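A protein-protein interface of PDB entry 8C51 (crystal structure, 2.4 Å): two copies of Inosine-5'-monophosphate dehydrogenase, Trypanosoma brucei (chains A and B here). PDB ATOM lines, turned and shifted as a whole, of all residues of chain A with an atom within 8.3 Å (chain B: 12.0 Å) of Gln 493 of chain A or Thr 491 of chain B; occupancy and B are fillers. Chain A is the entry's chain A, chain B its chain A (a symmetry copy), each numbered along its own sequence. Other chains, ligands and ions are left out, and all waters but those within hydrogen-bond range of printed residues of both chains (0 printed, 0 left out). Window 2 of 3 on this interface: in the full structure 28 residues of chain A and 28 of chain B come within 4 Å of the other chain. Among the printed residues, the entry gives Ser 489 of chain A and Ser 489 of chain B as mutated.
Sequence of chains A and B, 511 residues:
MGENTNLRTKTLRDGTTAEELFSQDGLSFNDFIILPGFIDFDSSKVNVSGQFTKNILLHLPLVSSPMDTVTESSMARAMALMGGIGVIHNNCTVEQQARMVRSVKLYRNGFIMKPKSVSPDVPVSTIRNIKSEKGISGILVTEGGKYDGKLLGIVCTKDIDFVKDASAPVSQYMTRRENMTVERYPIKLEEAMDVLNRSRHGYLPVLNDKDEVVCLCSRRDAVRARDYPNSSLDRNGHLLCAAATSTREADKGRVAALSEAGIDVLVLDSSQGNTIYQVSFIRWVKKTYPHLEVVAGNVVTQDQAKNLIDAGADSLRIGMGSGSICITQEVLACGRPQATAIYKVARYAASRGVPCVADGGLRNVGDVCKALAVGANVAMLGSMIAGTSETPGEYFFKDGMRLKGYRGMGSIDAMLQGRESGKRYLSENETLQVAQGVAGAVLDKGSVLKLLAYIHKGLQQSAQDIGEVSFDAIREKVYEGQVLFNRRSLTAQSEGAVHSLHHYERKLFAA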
ATOM      1  N   ASP A  25     -24.774  15.846 -10.023  1.00  0.00           N
ATOM      2  CA  ASP A  25     -25.607  16.951  -9.574  1.00  0.00           C
ATOM      3  C   ASP A  25     -24.745  18.122  -9.118  1.00  0.00           C
ATOM      4  O   ASP A  25     -23.551  17.980  -8.840  1.00  0.00           O
ATOM      5  CB  ASP A  25     -26.531  16.513  -8.435  1.00  0.00           C
ATOM      6  CG  ASP A  25     -25.846  15.586  -7.444  1.00  0.00           C
ATOM      7  OD1 ASP A  25     -26.023  15.788  -6.225  1.00  0.00           O
ATOM      8  OD2 ASP A  25     -25.134  14.656  -7.886  1.00  0.00           O
ATOM      9  N   GLY A  26     -25.372  19.293  -9.046  1.00  0.00           N
ATOM     10  CA  GLY A  26     -24.647  20.489  -8.654  1.00  0.00           C
ATOM     11  C   GLY A  26     -24.234  20.408  -7.196  1.00  0.00           C
ATOM     12  O   GLY A  26     -25.041  20.064  -6.324  1.00  0.00           O
ATOM     13  N   LEU A  27     -22.972  20.723  -6.928  1.00  0.00           N
ATOM     14  CA  LEU A  27     -22.387  20.571  -5.608  1.00  0.00           C
ATOM     15  C   LEU A  27     -22.027  21.924  -5.012  1.00  0.00           C
ATOM     16  O   LEU A  27     -21.696  22.875  -5.727  1.00  0.00           O
ATOM     17  CB  LEU A  27     -21.121  19.708  -5.662  1.00  0.00           C
ATOM     18  CG  LEU A  27     -21.215  18.361  -6.372  1.00  0.00           C
ATOM     19  CD1 LEU A  27     -19.857  17.682  -6.366  1.00  0.00           C
ATOM     20  CD2 LEU A  27     -22.260  17.480  -5.716  1.00  0.00           C
ATOM     21  N   SER A  28     -22.089  21.993  -3.686  1.00  0.00           N
ATOM     22  CA  SER A  28     -21.466  23.060  -2.927  1.00  0.00           C
ATOM     23  C   SER A  28     -20.168  22.525  -2.328  1.00  0.00           C
ATOM     24  O   SER A  28     -19.816  21.355  -2.486  1.00  0.00           O
ATOM     25  CB  SER A  28     -22.406  23.584  -1.846  1.00  0.00           C
ATOM     26  OG  SER A  28     -22.287  22.806  -0.672  1.00  0.00           O
ATOM     27  N   PHE A  29     -19.459  23.389  -1.602  1.00  0.00           N
ATOM     28  CA  PHE A  29     -18.113  23.047  -1.159  1.00  0.00           C
ATOM     29  C   PHE A  29     -18.084  21.991  -0.061  1.00  0.00           C
ATOM     30  O   PHE A  29     -17.072  21.294   0.073  1.00  0.00           O
ATOM     31  CB  PHE A  29     -17.405  24.313  -0.685  1.00  0.00           C
ATOM     32  CG  PHE A  29     -17.252  25.342  -1.758  1.00  0.00           C
ATOM     33  CD1 PHE A  29     -16.585  25.037  -2.930  1.00  0.00           C
ATOM     34  CD2 PHE A  29     -17.795  26.604  -1.608  1.00  0.00           C
ATOM     35  CE1 PHE A  29     -16.449  25.973  -3.927  1.00  0.00           C
ATOM     36  CE2 PHE A  29     -17.663  27.547  -2.601  1.00  0.00           C
ATOM     37  CZ  PHE A  29     -16.990  27.232  -3.763  1.00  0.00           C
ATOM     38  N   ASN A  30     -19.156  21.845   0.713  1.00  0.00           N
ATOM     39  CA  ASN A  30     -19.189  20.838   1.765  1.00  0.00           C
ATOM     40  C   ASN A  30     -19.433  19.431   1.233  1.00  0.00           C
ATOM     41  O   ASN A  30     -19.271  18.467   1.988  1.00  0.00           O
ATOM     42  CB  ASN A  30     -20.272  21.184   2.792  1.00  0.00           C
ATOM     43  CG  ASN A  30     -19.850  22.288   3.745  1.00  0.00           C
ATOM     44  OD1 ASN A  30     -18.666  22.460   4.034  1.00  0.00           O
ATOM     45  ND2 ASN A  30     -20.824  23.045   4.238  1.00  0.00           N
ATOM     46  N   ASP A  31     -19.821  19.290  -0.036  1.00  0.00           N
ATOM     47  CA  ASP A  31     -20.146  17.986  -0.599  1.00  0.00           C
ATOM     48  C   ASP A  31     -18.918  17.147  -0.920  1.00  0.00           C
ATOM     49  O   ASP A  31     -19.064  15.954  -1.206  1.00  0.00           O
ATOM     50  CB  ASP A  31     -20.973  18.163  -1.876  1.00  0.00           C
ATOM     51  CG  ASP A  31     -22.430  18.461  -1.597  1.00  0.00           C
ATOM     52  OD1 ASP A  31     -22.985  19.352  -2.276  1.00  0.00           O
ATOM     53  OD2 ASP A  31     -23.025  17.799  -0.719  1.00  0.00           O
ATOM     54  N   PHE A  32     -17.725  17.731  -0.892  1.00  0.00           N
ATOM     55  CA  PHE A  32     -16.528  17.008  -1.288  1.00  0.00           C
ATOM     56  C   PHE A  32     -15.343  17.486  -0.463  1.00  0.00           C
ATOM     57  O   PHE A  32     -15.375  18.554   0.154  1.00  0.00           O
ATOM     58  CB  PHE A  32     -16.238  17.183  -2.783  1.00  0.00           C
ATOM     59  CG  PHE A  32     -15.857  18.583  -3.164  1.00  0.00           C
ATOM     60  CD1 PHE A  32     -16.828  19.510  -3.496  1.00  0.00           C
ATOM     61  CD2 PHE A  32     -14.529  18.971  -3.193  1.00  0.00           C
ATOM     62  CE1 PHE A  32     -16.484  20.797  -3.850  1.00  0.00           C
ATOM     63  CE2 PHE A  32     -14.178  20.258  -3.547  1.00  0.00           C
ATOM     64  CZ  PHE A  32     -15.157  21.172  -3.875  1.00  0.00           C
ATOM     65  N   ILE A  33     -14.289  16.673  -0.470  1.00  0.00           N
ATOM     66  CA  ILE A  33     -13.043  16.993   0.210  1.00  0.00           C
ATOM     67  C   ILE A  33     -11.889  16.628  -0.713  1.00  0.00           C
ATOM     68  O   ILE A  33     -12.021  15.781  -1.603  1.00  0.00           O
ATOM     69  CB  ILE A  33     -12.915  16.263   1.567  1.00  0.00           C
ATOM     70  CG1 ILE A  33     -11.843  16.922   2.438  1.00  0.00           C
ATOM     71  CG2 ILE A  33     -12.605  14.786   1.356  1.00  0.00           C
ATOM     72  CD1 ILE A  33     -11.828  16.412   3.864  1.00  0.00           C
ATOM     73  N   PRO A 337     -25.573  25.776  -7.938  1.00  0.00           N
ATOM     74  CA  PRO A 337     -24.639  25.461  -6.850  1.00  0.00           C
ATOM     75  C   PRO A 337     -23.227  25.933  -7.172  1.00  0.00           C
ATOM     76  O   PRO A 337     -22.731  25.763  -8.287  1.00  0.00           O
ATOM     77  CB  PRO A 337     -24.723  23.936  -6.746  1.00  0.00           C
ATOM     78  CG  PRO A 337     -26.114  23.616  -7.184  1.00  0.00           C
ATOM     79  CD  PRO A 337     -26.525  24.674  -8.181  1.00  0.00           C
ATOM     80  N   LYS A 370     -10.866  25.211  -1.400  1.00  0.00           N
ATOM     81  CA  LYS A 370     -11.549  24.355  -2.364  1.00  0.00           C
ATOM     82  C   LYS A 370     -11.884  25.118  -3.640  1.00  0.00           C
ATOM     83  O   LYS A 370     -11.679  24.614  -4.749  1.00  0.00           O
ATOM     84  CB  LYS A 370     -12.821  23.777  -1.742  1.00  0.00           C
ATOM     85  CG  LYS A 370     -12.572  22.743  -0.661  1.00  0.00           C
ATOM     86  CD  LYS A 370     -13.875  22.258  -0.046  1.00  0.00           C
ATOM     87  CE  LYS A 370     -13.621  21.324   1.125  1.00  0.00           C
ATOM     88  NZ  LYS A 370     -14.869  21.006   1.868  1.00  0.00           N
ATOM     89  N   ARG A 487     -16.122  12.664  -2.933  1.00  0.00           N
ATOM     90  CA  ARG A 487     -17.441  13.154  -2.573  1.00  0.00           C
ATOM     91  C   ARG A 487     -17.824  12.595  -1.210  1.00  0.00           C
ATOM     92  O   ARG A 487     -17.558  11.429  -0.903  1.00  0.00           O
ATOM     93  CB  ARG A 487     -18.465  12.743  -3.627  1.00  0.00           C
ATOM     94  CG  ARG A 487     -19.891  13.093  -3.263  1.00  0.00           C
ATOM     95  CD  ARG A 487     -20.638  13.653  -4.452  1.00  0.00           C
ATOM     96  NE  ARG A 487     -21.974  14.103  -4.084  1.00  0.00           N
ATOM     97  CZ  ARG A 487     -22.990  14.212  -4.927  1.00  0.00           C
ATOM     98  NH1 ARG A 487     -22.864  13.905  -6.208  1.00  0.00           N
ATOM     99  NH2 ARG A 487     -24.165  14.640  -4.474  1.00  0.00           N
ATOM    100  N   ARG A 488     -18.445  13.432  -0.389  1.00  0.00           N
ATOM    101  CA  ARG A 488     -18.813  13.067   0.970  1.00  0.00           C
ATOM    102  C   ARG A 488     -20.311  12.827   1.052  1.00  0.00           C
ATOM    103  O   ARG A 488     -21.105  13.698   0.683  1.00  0.00           O
ATOM    104  CB  ARG A 488     -18.406  14.163   1.954  1.00  0.00           C
ATOM    105  CG  ARG A 488     -17.032  14.740   1.682  1.00  0.00           C
ATOM    106  CD  ARG A 488     -16.387  15.242   2.958  1.00  0.00           C
ATOM    107  NE  ARG A 488     -16.873  16.566   3.321  1.00  0.00           N
ATOM    108  CZ  ARG A 488     -16.925  17.034   4.561  1.00  0.00           C
ATOM    109  NH1 ARG A 488     -16.525  16.307   5.592  1.00  0.00           N
ATOM    110  NH2 ARG A 488     -17.393  18.260   4.772  1.00  0.00           N
ATOM    111  N   SER A 489     -20.692  11.650   1.535  1.00  0.00           N
ATOM    112  CA  SER A 489     -22.090  11.398   1.833  1.00  0.00           C
ATOM    113  C   SER A 489     -22.582  12.403   2.868  1.00  0.00           C
ATOM    114  O   SER A 489     -21.799  13.015   3.598  1.00  0.00           O
ATOM    115  CB  SER A 489     -22.278   9.977   2.354  1.00  0.00           C
ATOM    116  OG  SER A 489     -21.672   9.829   3.626  1.00  0.00           O
ATOM    117  N   LEU A 490     -23.903  12.568   2.931  1.00  0.00           N
ATOM    118  CA  LEU A 490     -24.463  13.517   3.887  1.00  0.00           C
ATOM    119  C   LEU A 490     -24.055  13.150   5.307  1.00  0.00           C
ATOM    120  O   LEU A 490     -23.801  14.030   6.137  1.00  0.00           O
ATOM    121  CB  LEU A 490     -25.984  13.565   3.756  1.00  0.00           C
ATOM    122  N   THR A 491     -23.969  11.851   5.598  1.00  0.00           N
ATOM    123  CA  THR A 491     -23.527  11.417   6.919  1.00  0.00           C
ATOM    124  C   THR A 491     -22.061  11.759   7.149  1.00  0.00           C
ATOM    125  O   THR A 491     -21.678  12.157   8.256  1.00  0.00           O
ATOM    126  CB  THR A 491     -23.765   9.911   7.068  1.00  0.00           C
ATOM    127  OG1 THR A 491     -25.169   9.660   7.207  1.00  0.00           O
ATOM    128  CG2 THR A 491     -23.042   9.336   8.288  1.00  0.00           C
ATOM    129  N   ALA A 492     -21.224  11.615   6.119  1.00  0.00           N
ATOM    130  CA  ALA A 492     -19.792  11.844   6.268  1.00  0.00           C
ATOM    131  C   ALA A 492     -19.446  13.292   6.586  1.00  0.00           C
ATOM    132  O   ALA A 492     -18.272  13.585   6.826  1.00  0.00           O
ATOM    133  CB  ALA A 492     -19.056  11.413   4.998  1.00  0.00           C
ATOM    134  N   GLN A 493     -20.423  14.195   6.591  1.00  0.00           N
ATOM    135  CA  GLN A 493     -20.196  15.600   6.934  1.00  0.00           C
ATOM    136  C   GLN A 493     -20.585  15.888   8.381  1.00  0.00           C
ATOM    137  O   GLN A 493     -21.291  16.855   8.671  1.00  0.00           O
ATOM    138  CB  GLN A 493     -20.961  16.505   5.975  1.00  0.00           C
ATOM    139  CG  GLN A 493     -20.849  16.101   4.507  1.00  0.00           C
ATOM    140  CD  GLN A 493     -21.722  16.949   3.595  1.00  0.00           C
ATOM    141  OE1 GLN A 493     -22.135  18.050   3.958  1.00  0.00           O
ATOM    142  NE2 GLN A 493     -22.010  16.433   2.404  1.00  0.00           N
ATOM    143  N   SER A 494     -20.135  15.047   9.307  1.00  0.00           N
ATOM    144  CA  SER A 494     -20.416  15.244  10.727  1.00  0.00           C
ATOM    145  C   SER A 494     -19.254  14.756  11.585  1.00  0.00           C
ATOM    146  O   SER A 494     -18.096  15.070  11.316  1.00  0.00           O
ATOM    147  CB  SER A 494     -21.703  14.523  11.125  1.00  0.00           C
ATOM    148  OG  SER A 494     -22.794  14.960  10.335  1.00  0.00           O
ATOM    149  N   ASN B  30     -37.511  22.038  -4.752  1.00  0.00           N
ATOM    150  CA  ASN B  30     -36.259  22.466  -4.144  1.00  0.00           C
ATOM    151  C   ASN B  30     -35.069  21.618  -4.577  1.00  0.00           C
ATOM    152  O   ASN B  30     -33.927  22.004  -4.307  1.00  0.00           O
ATOM    153  CB  ASN B  30     -36.374  22.429  -2.617  1.00  0.00           C
ATOM    154  CG  ASN B  30     -37.148  23.610  -2.056  1.00  0.00           C
ATOM    155  OD1 ASN B  30     -37.163  24.694  -2.638  1.00  0.00           O
ATOM    156  ND2 ASN B  30     -37.798  23.400  -0.917  1.00  0.00           N
ATOM    157  N   ASP B  31     -35.304  20.479  -5.232  1.00  0.00           N
ATOM    158  CA  ASP B  31     -34.227  19.577  -5.616  1.00  0.00           C
ATOM    159  C   ASP B  31     -33.434  20.063  -6.820  1.00  0.00           C
ATOM    160  O   ASP B  31     -32.377  19.496  -7.112  1.00  0.00           O
ATOM    161  CB  ASP B  31     -34.795  18.189  -5.924  1.00  0.00           C
ATOM    162  CG  ASP B  31     -35.093  17.385  -4.677  1.00  0.00           C
ATOM    163  OD1 ASP B  31     -36.168  16.748  -4.635  1.00  0.00           O
ATOM    164  OD2 ASP B  31     -34.253  17.372  -3.751  1.00  0.00           O
ATOM    165  N   PHE B  32     -33.915  21.080  -7.528  1.00  0.00           N
ATOM    166  CA  PHE B  32     -33.258  21.522  -8.747  1.00  0.00           C
ATOM    167  C   PHE B  32     -33.419  23.026  -8.901  1.00  0.00           C
ATOM    168  O   PHE B  32     -34.278  23.650  -8.271  1.00  0.00           O
ATOM    169  CB  PHE B  32     -33.818  20.800  -9.977  1.00  0.00           C
ATOM    170  CG  PHE B  32     -35.243  21.151 -10.287  1.00  0.00           C
ATOM    171  CD1 PHE B  32     -36.282  20.447  -9.707  1.00  0.00           C
ATOM    172  CD2 PHE B  32     -35.544  22.183 -11.158  1.00  0.00           C
ATOM    173  CE1 PHE B  32     -37.594  20.763  -9.989  1.00  0.00           C
ATOM    174  CE2 PHE B  32     -36.854  22.505 -11.445  1.00  0.00           C
ATOM    175  CZ  PHE B  32     -37.881  21.794 -10.860  1.00  0.00           C
ATOM    176  N   ILE B  33     -32.577  23.597  -9.759  1.00  0.00           N
ATOM    177  CA  ILE B  33     -32.623  25.015 -10.083  1.00  0.00           C
ATOM    178  C   ILE B  33     -32.456  25.165 -11.588  1.00  0.00           C
ATOM    179  O   ILE B  33     -31.894  24.295 -12.263  1.00  0.00           O
ATOM    180  CB  ILE B  33     -31.543  25.821  -9.325  1.00  0.00           C
ATOM    181  CG1 ILE B  33     -31.872  27.316  -9.340  1.00  0.00           C
ATOM    182  CG2 ILE B  33     -30.164  25.567  -9.923  1.00  0.00           C
ATOM    183  CD1 ILE B  33     -30.991  28.136  -8.421  1.00  0.00           C
ATOM    184  N   ASN B 486     -29.971  22.308 -13.117  1.00  0.00           N
ATOM    185  CA  ASN B 486     -28.983  21.618 -12.307  1.00  0.00           C
ATOM    186  C   ASN B 486     -29.692  21.039 -11.098  1.00  0.00           C
ATOM    187  O   ASN B 486     -30.403  21.757 -10.387  1.00  0.00           O
ATOM    188  CB  ASN B 486     -27.852  22.548 -11.867  1.00  0.00           C
ATOM    189  CG  ASN B 486     -26.520  22.164 -12.473  1.00  0.00           C
ATOM    190  OD1 ASN B 486     -26.455  21.665 -13.599  1.00  0.00           O
ATOM    191  ND2 ASN B 486     -25.450  22.376 -11.724  1.00  0.00           N
ATOM    192  N   ARG B 487     -29.514  19.742 -10.881  1.00  0.00           N
ATOM    193  CA  ARG B 487     -29.965  19.134  -9.642  1.00  0.00           C
ATOM    194  C   ARG B 487     -29.079  19.615  -8.502  1.00  0.00           C
ATOM    195  O   ARG B 487     -27.860  19.738  -8.652  1.00  0.00           O
ATOM    196  CB  ARG B 487     -29.921  17.613  -9.750  1.00  0.00           C
ATOM    197  CG  ARG B 487     -30.243  16.899  -8.456  1.00  0.00           C
ATOM    198  CD  ARG B 487     -31.153  15.715  -8.696  1.00  0.00           C
ATOM    199  NE  ARG B 487     -31.563  15.091  -7.446  1.00  0.00           N
ATOM    200  CZ  ARG B 487     -31.961  13.832  -7.328  1.00  0.00           C
ATOM    201  NH1 ARG B 487     -32.009  13.020  -8.371  1.00  0.00           N
ATOM    202  NH2 ARG B 487     -32.318  13.376  -6.131  1.00  0.00           N
ATOM    203  N   ARG B 488     -29.695  19.893  -7.360  1.00  0.00           N
ATOM    204  CA  ARG B 488     -28.995  20.426  -6.202  1.00  0.00           C
ATOM    205  C   ARG B 488     -28.832  19.340  -5.152  1.00  0.00           C
ATOM    206  O   ARG B 488     -29.817  18.726  -4.729  1.00  0.00           O
ATOM    207  CB  ARG B 488     -29.752  21.613  -5.610  1.00  0.00           C
ATOM    208  CG  ARG B 488     -30.298  22.564  -6.656  1.00  0.00           C
ATOM    209  CD  ARG B 488     -30.391  23.977  -6.115  1.00  0.00           C
ATOM    210  NE  ARG B 488     -31.592  24.167  -5.313  1.00  0.00           N
ATOM    211  CZ  ARG B 488     -31.705  25.044  -4.324  1.00  0.00           C
ATOM    212  NH1 ARG B 488     -30.700  25.836  -3.985  1.00  0.00           N
ATOM    213  NH2 ARG B 488     -32.852  25.125  -3.658  1.00  0.00           N
ATOM    214  N   SER B 489     -27.593  19.106  -4.736  1.00  0.00           N
ATOM    215  CA  SER B 489     -27.354  18.230  -3.604  1.00  0.00           C
ATOM    216  C   SER B 489     -28.064  18.778  -2.372  1.00  0.00           C
ATOM    217  O   SER B 489     -28.405  19.962  -2.295  1.00  0.00           O
ATOM    218  CB  SER B 489     -25.858  18.104  -3.331  1.00  0.00           C
ATOM    219  OG  SER B 489     -25.332  19.335  -2.869  1.00  0.00           O
ATOM    220  N   LEU B 490     -28.285  17.902  -1.393  1.00  0.00           N
ATOM    221  CA  LEU B 490     -28.968  18.337  -0.180  1.00  0.00           C
ATOM    222  C   LEU B 490     -28.203  19.471   0.488  1.00  0.00           C
ATOM    223  O   LEU B 490     -28.804  20.398   1.042  1.00  0.00           O
ATOM    224  CB  LEU B 490     -29.142  17.162   0.781  1.00  0.00           C
ATOM    225  N   THR B 491     -26.870  19.423   0.429  1.00  0.00           N
ATOM    226  CA  THR B 491     -26.066  20.501   0.992  1.00  0.00           C
ATOM    227  C   THR B 491     -26.242  21.791   0.202  1.00  0.00           C
ATOM    228  O   THR B 491     -26.298  22.879   0.786  1.00  0.00           O
ATOM    229  CB  THR B 491     -24.594  20.078   1.022  1.00  0.00           C
ATOM    230  OG1 THR B 491     -24.399  19.094   2.045  1.00  0.00           O
ATOM    231  CG2 THR B 491     -23.664  21.261   1.298  1.00  0.00           C
ATOM    232  N   ALA B 492     -26.336  21.693  -1.126  1.00  0.00           N
ATOM    233  CA  ALA B 492     -26.428  22.880  -1.969  1.00  0.00           C
ATOM    234  C   ALA B 492     -27.711  23.671  -1.751  1.00  0.00           C
ATOM    235  O   ALA B 492     -27.855  24.745  -2.342  1.00  0.00           O
ATOM    236  CB  ALA B 492     -26.318  22.487  -3.443  1.00  0.00           C
ATOM    237  N   GLN B 493     -28.635  23.176  -0.932  1.00  0.00           N
ATOM    238  CA  GLN B 493     -29.875  23.888  -0.622  1.00  0.00           C
ATOM    239  C   GLN B 493     -29.780  24.614   0.716  1.00  0.00           C
ATOM    240  O   GLN B 493     -30.671  24.514   1.561  1.00  0.00           O
ATOM    241  CB  GLN B 493     -31.053  22.919  -0.632  1.00  0.00           C
ATOM    242  CG  GLN B 493     -31.061  21.953  -1.813  1.00  0.00           C
ATOM    243  CD  GLN B 493     -32.177  20.924  -1.725  1.00  0.00           C
ATOM    244  OE1 GLN B 493     -33.159  21.115  -1.009  1.00  0.00           O
ATOM    245  NE2 GLN B 493     -32.025  19.822  -2.453  1.00  0.00           N
ATOM    246  N   SER B 494     -28.691  25.347   0.930  1.00  0.00           N
ATOM    247  CA  SER B 494     -28.509  26.112   2.161  1.00  0.00           C
ATOM    248  C   SER B 494     -27.735  27.398   1.892  1.00  0.00           C
ATOM    249  O   SER B 494     -28.040  28.134   0.955  1.00  0.00           O
ATOM    250  CB  SER B 494     -27.785  25.274   3.213  1.00  0.00           C
ATOM    251  OG  SER B 494     -28.487  24.071   3.472  1.00  0.00           O
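The side-chain hydroxyl of Thr 491 of chain B lies close to the side-chain carboxylate of Asp 31 of chain A, 3.3 Å away.
The side-chain amide oxygen (OE1) of Gln 493 of chain A lies within hydrogen-bond range of the side-chain hydroxyl (OG1) of Thr 491 of chain B, at 3.1 Å.
The backbone NH of Gly 26 of chain A is in hydrogen-bond range of the backbone carbonyl oxygen of Arg 487 of chain B (2.6 Å).
The side-chain hydroxyl (OG) of Ser 489 of chain B lies within hydrogen-bond range of the side-chain carboxylate (OD1) of Asp 31 of chain A (2.4 Å).
O of Gly 26 of chain A sits at hydrogen-bond distance from N of Ser 489 of chain B, at 3.2 Å.
The backbone NH (N) of Ser 28 of chain A lies within hydrogen-bond range of the side-chain carboxylate (OD1) of Asp 31 of chain A (3.1 Å).
The side-chain hydroxyl of Ser 489 of chain B sits at hydrogen-bond distance from the backbone NH of Ala 492 of chain B.
O of Asp 31 of chain A sits at hydrogen-bond distance from N of Arg 488 of chain A, at 2.7 Å.
O of Arg 488 of chain A lies within hydrogen-bond range of NE2 of Gln 493 of chain A (3.4 Å).
The backbone carbonyl oxygen (O) of Arg 488 of chain B is in hydrogen-bond range of the side-chain amide nitrogen (NE2) of Gln 493 of chain B, at 3.4 Å.
N of Arg 488 of chain B lies within hydrogen-bond range of O of Asp 31 of chain B.
Among the printed residues, merely in contact across the chains: Asp 25 of chain A with Arg 487 of chain B (3.5 Å), Asp 25 of chain A with Ser 489 of chain B (3.7 Å), Gly 26 of chain A with Asn 486 of chain B (3.7 Å), Gly 26 of chain A with Arg 488 of chain B (3.97 Å), Gly 26 of chain A with Ala 492 of chain B (3.98 Å), Ser 28 of chain A with Thr 491 of chain B (2.9 Å), Asn 30 of chain A with Thr 491 of chain B (3.7 Å) and Pro 337 of chain A with Ala 492 of chain B (3.9 Å).
Printed residues of chain B within 4 Å of Ser 28 of chain A: Thr 491 (2.9 Å).
Asn 30 of chain A touches just one residue of chain B: Thr 491 (3.7 Å).
Asp 31 of chain A touches just these residues of chain B: Ser 489 and Thr 491.
Printed residues of chain B within 4 Å of Pro 337 of chain A: Ala 492 (3.9 Å).
No residue of chain B comes within 4 Å of Arg 488 of chain A.
No residue of chain B comes within 4 Å of Ser 489 of chain A.
No residue of chain B comes within 4 Å of Thr 491 of chain A.
Gln 493 of chain A touches just one residue of chain B: Thr 491 (3.1 Å).
Printed residues of chain A within 4 Å of Arg 487 of chain B: Asp 25 (3.5 Å) and Gly 26 (2.6 Å).
Printed residues of chain A within 4 Å of Arg 488 of chain B: Gly 26.
No residue of chain A comes within 4 Å of Leu 490 of chain B.
Of chain A, only Ser 28, Asn 30, Asp 31 and Gln 493 come within 4 Å of Thr 491 of chain B.
Ala 492 of chain B touches just these residues of chain A: Gly 26 (3.98 Å) and Pro 337 (3.9 Å).
The nearest residue of chain B that does not touch Gln 493 of chain A is Ser 489 of chain B (6.9 Å).
The nearest residue of chain A that does not touch Thr 491 of chain B is Phe 29 of chain A (5.5 Å).
Of the 13 printed residues of chain B, 6 touch a printed residue of chain A.
Hydrophobic or aromatic side chains of chain B that line the printed part of chain A: Ala 492.
Asn 30 of chain A touches Thr 491 of chain B, but with the chains exchanged Thr 491 of chain A does not touch Asn 30 of chain B (17.3 Å).
Asp 31 of chain A touches Ser 489 of chain B, but with the chains exchanged Ser 489 of chain A does not touch Asp 31 of chain B (14.3 Å).
Asp 31 of chain A touches Thr 491 of chain B, but with the chains exchanged Thr 491 of chain A does not touch Asp 31 of chain B (15.0 Å).
Gln 493 of chain A touches Thr 491 of chain B, but with the chains exchanged Thr 491 of chain A does not touch Gln 493 of chain B (13.9 Å).
12 positions are printed for both chains.
Of the 13 pairs that touch across the chains among the printed residues, none has its exchanged pair printed and touching as well.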
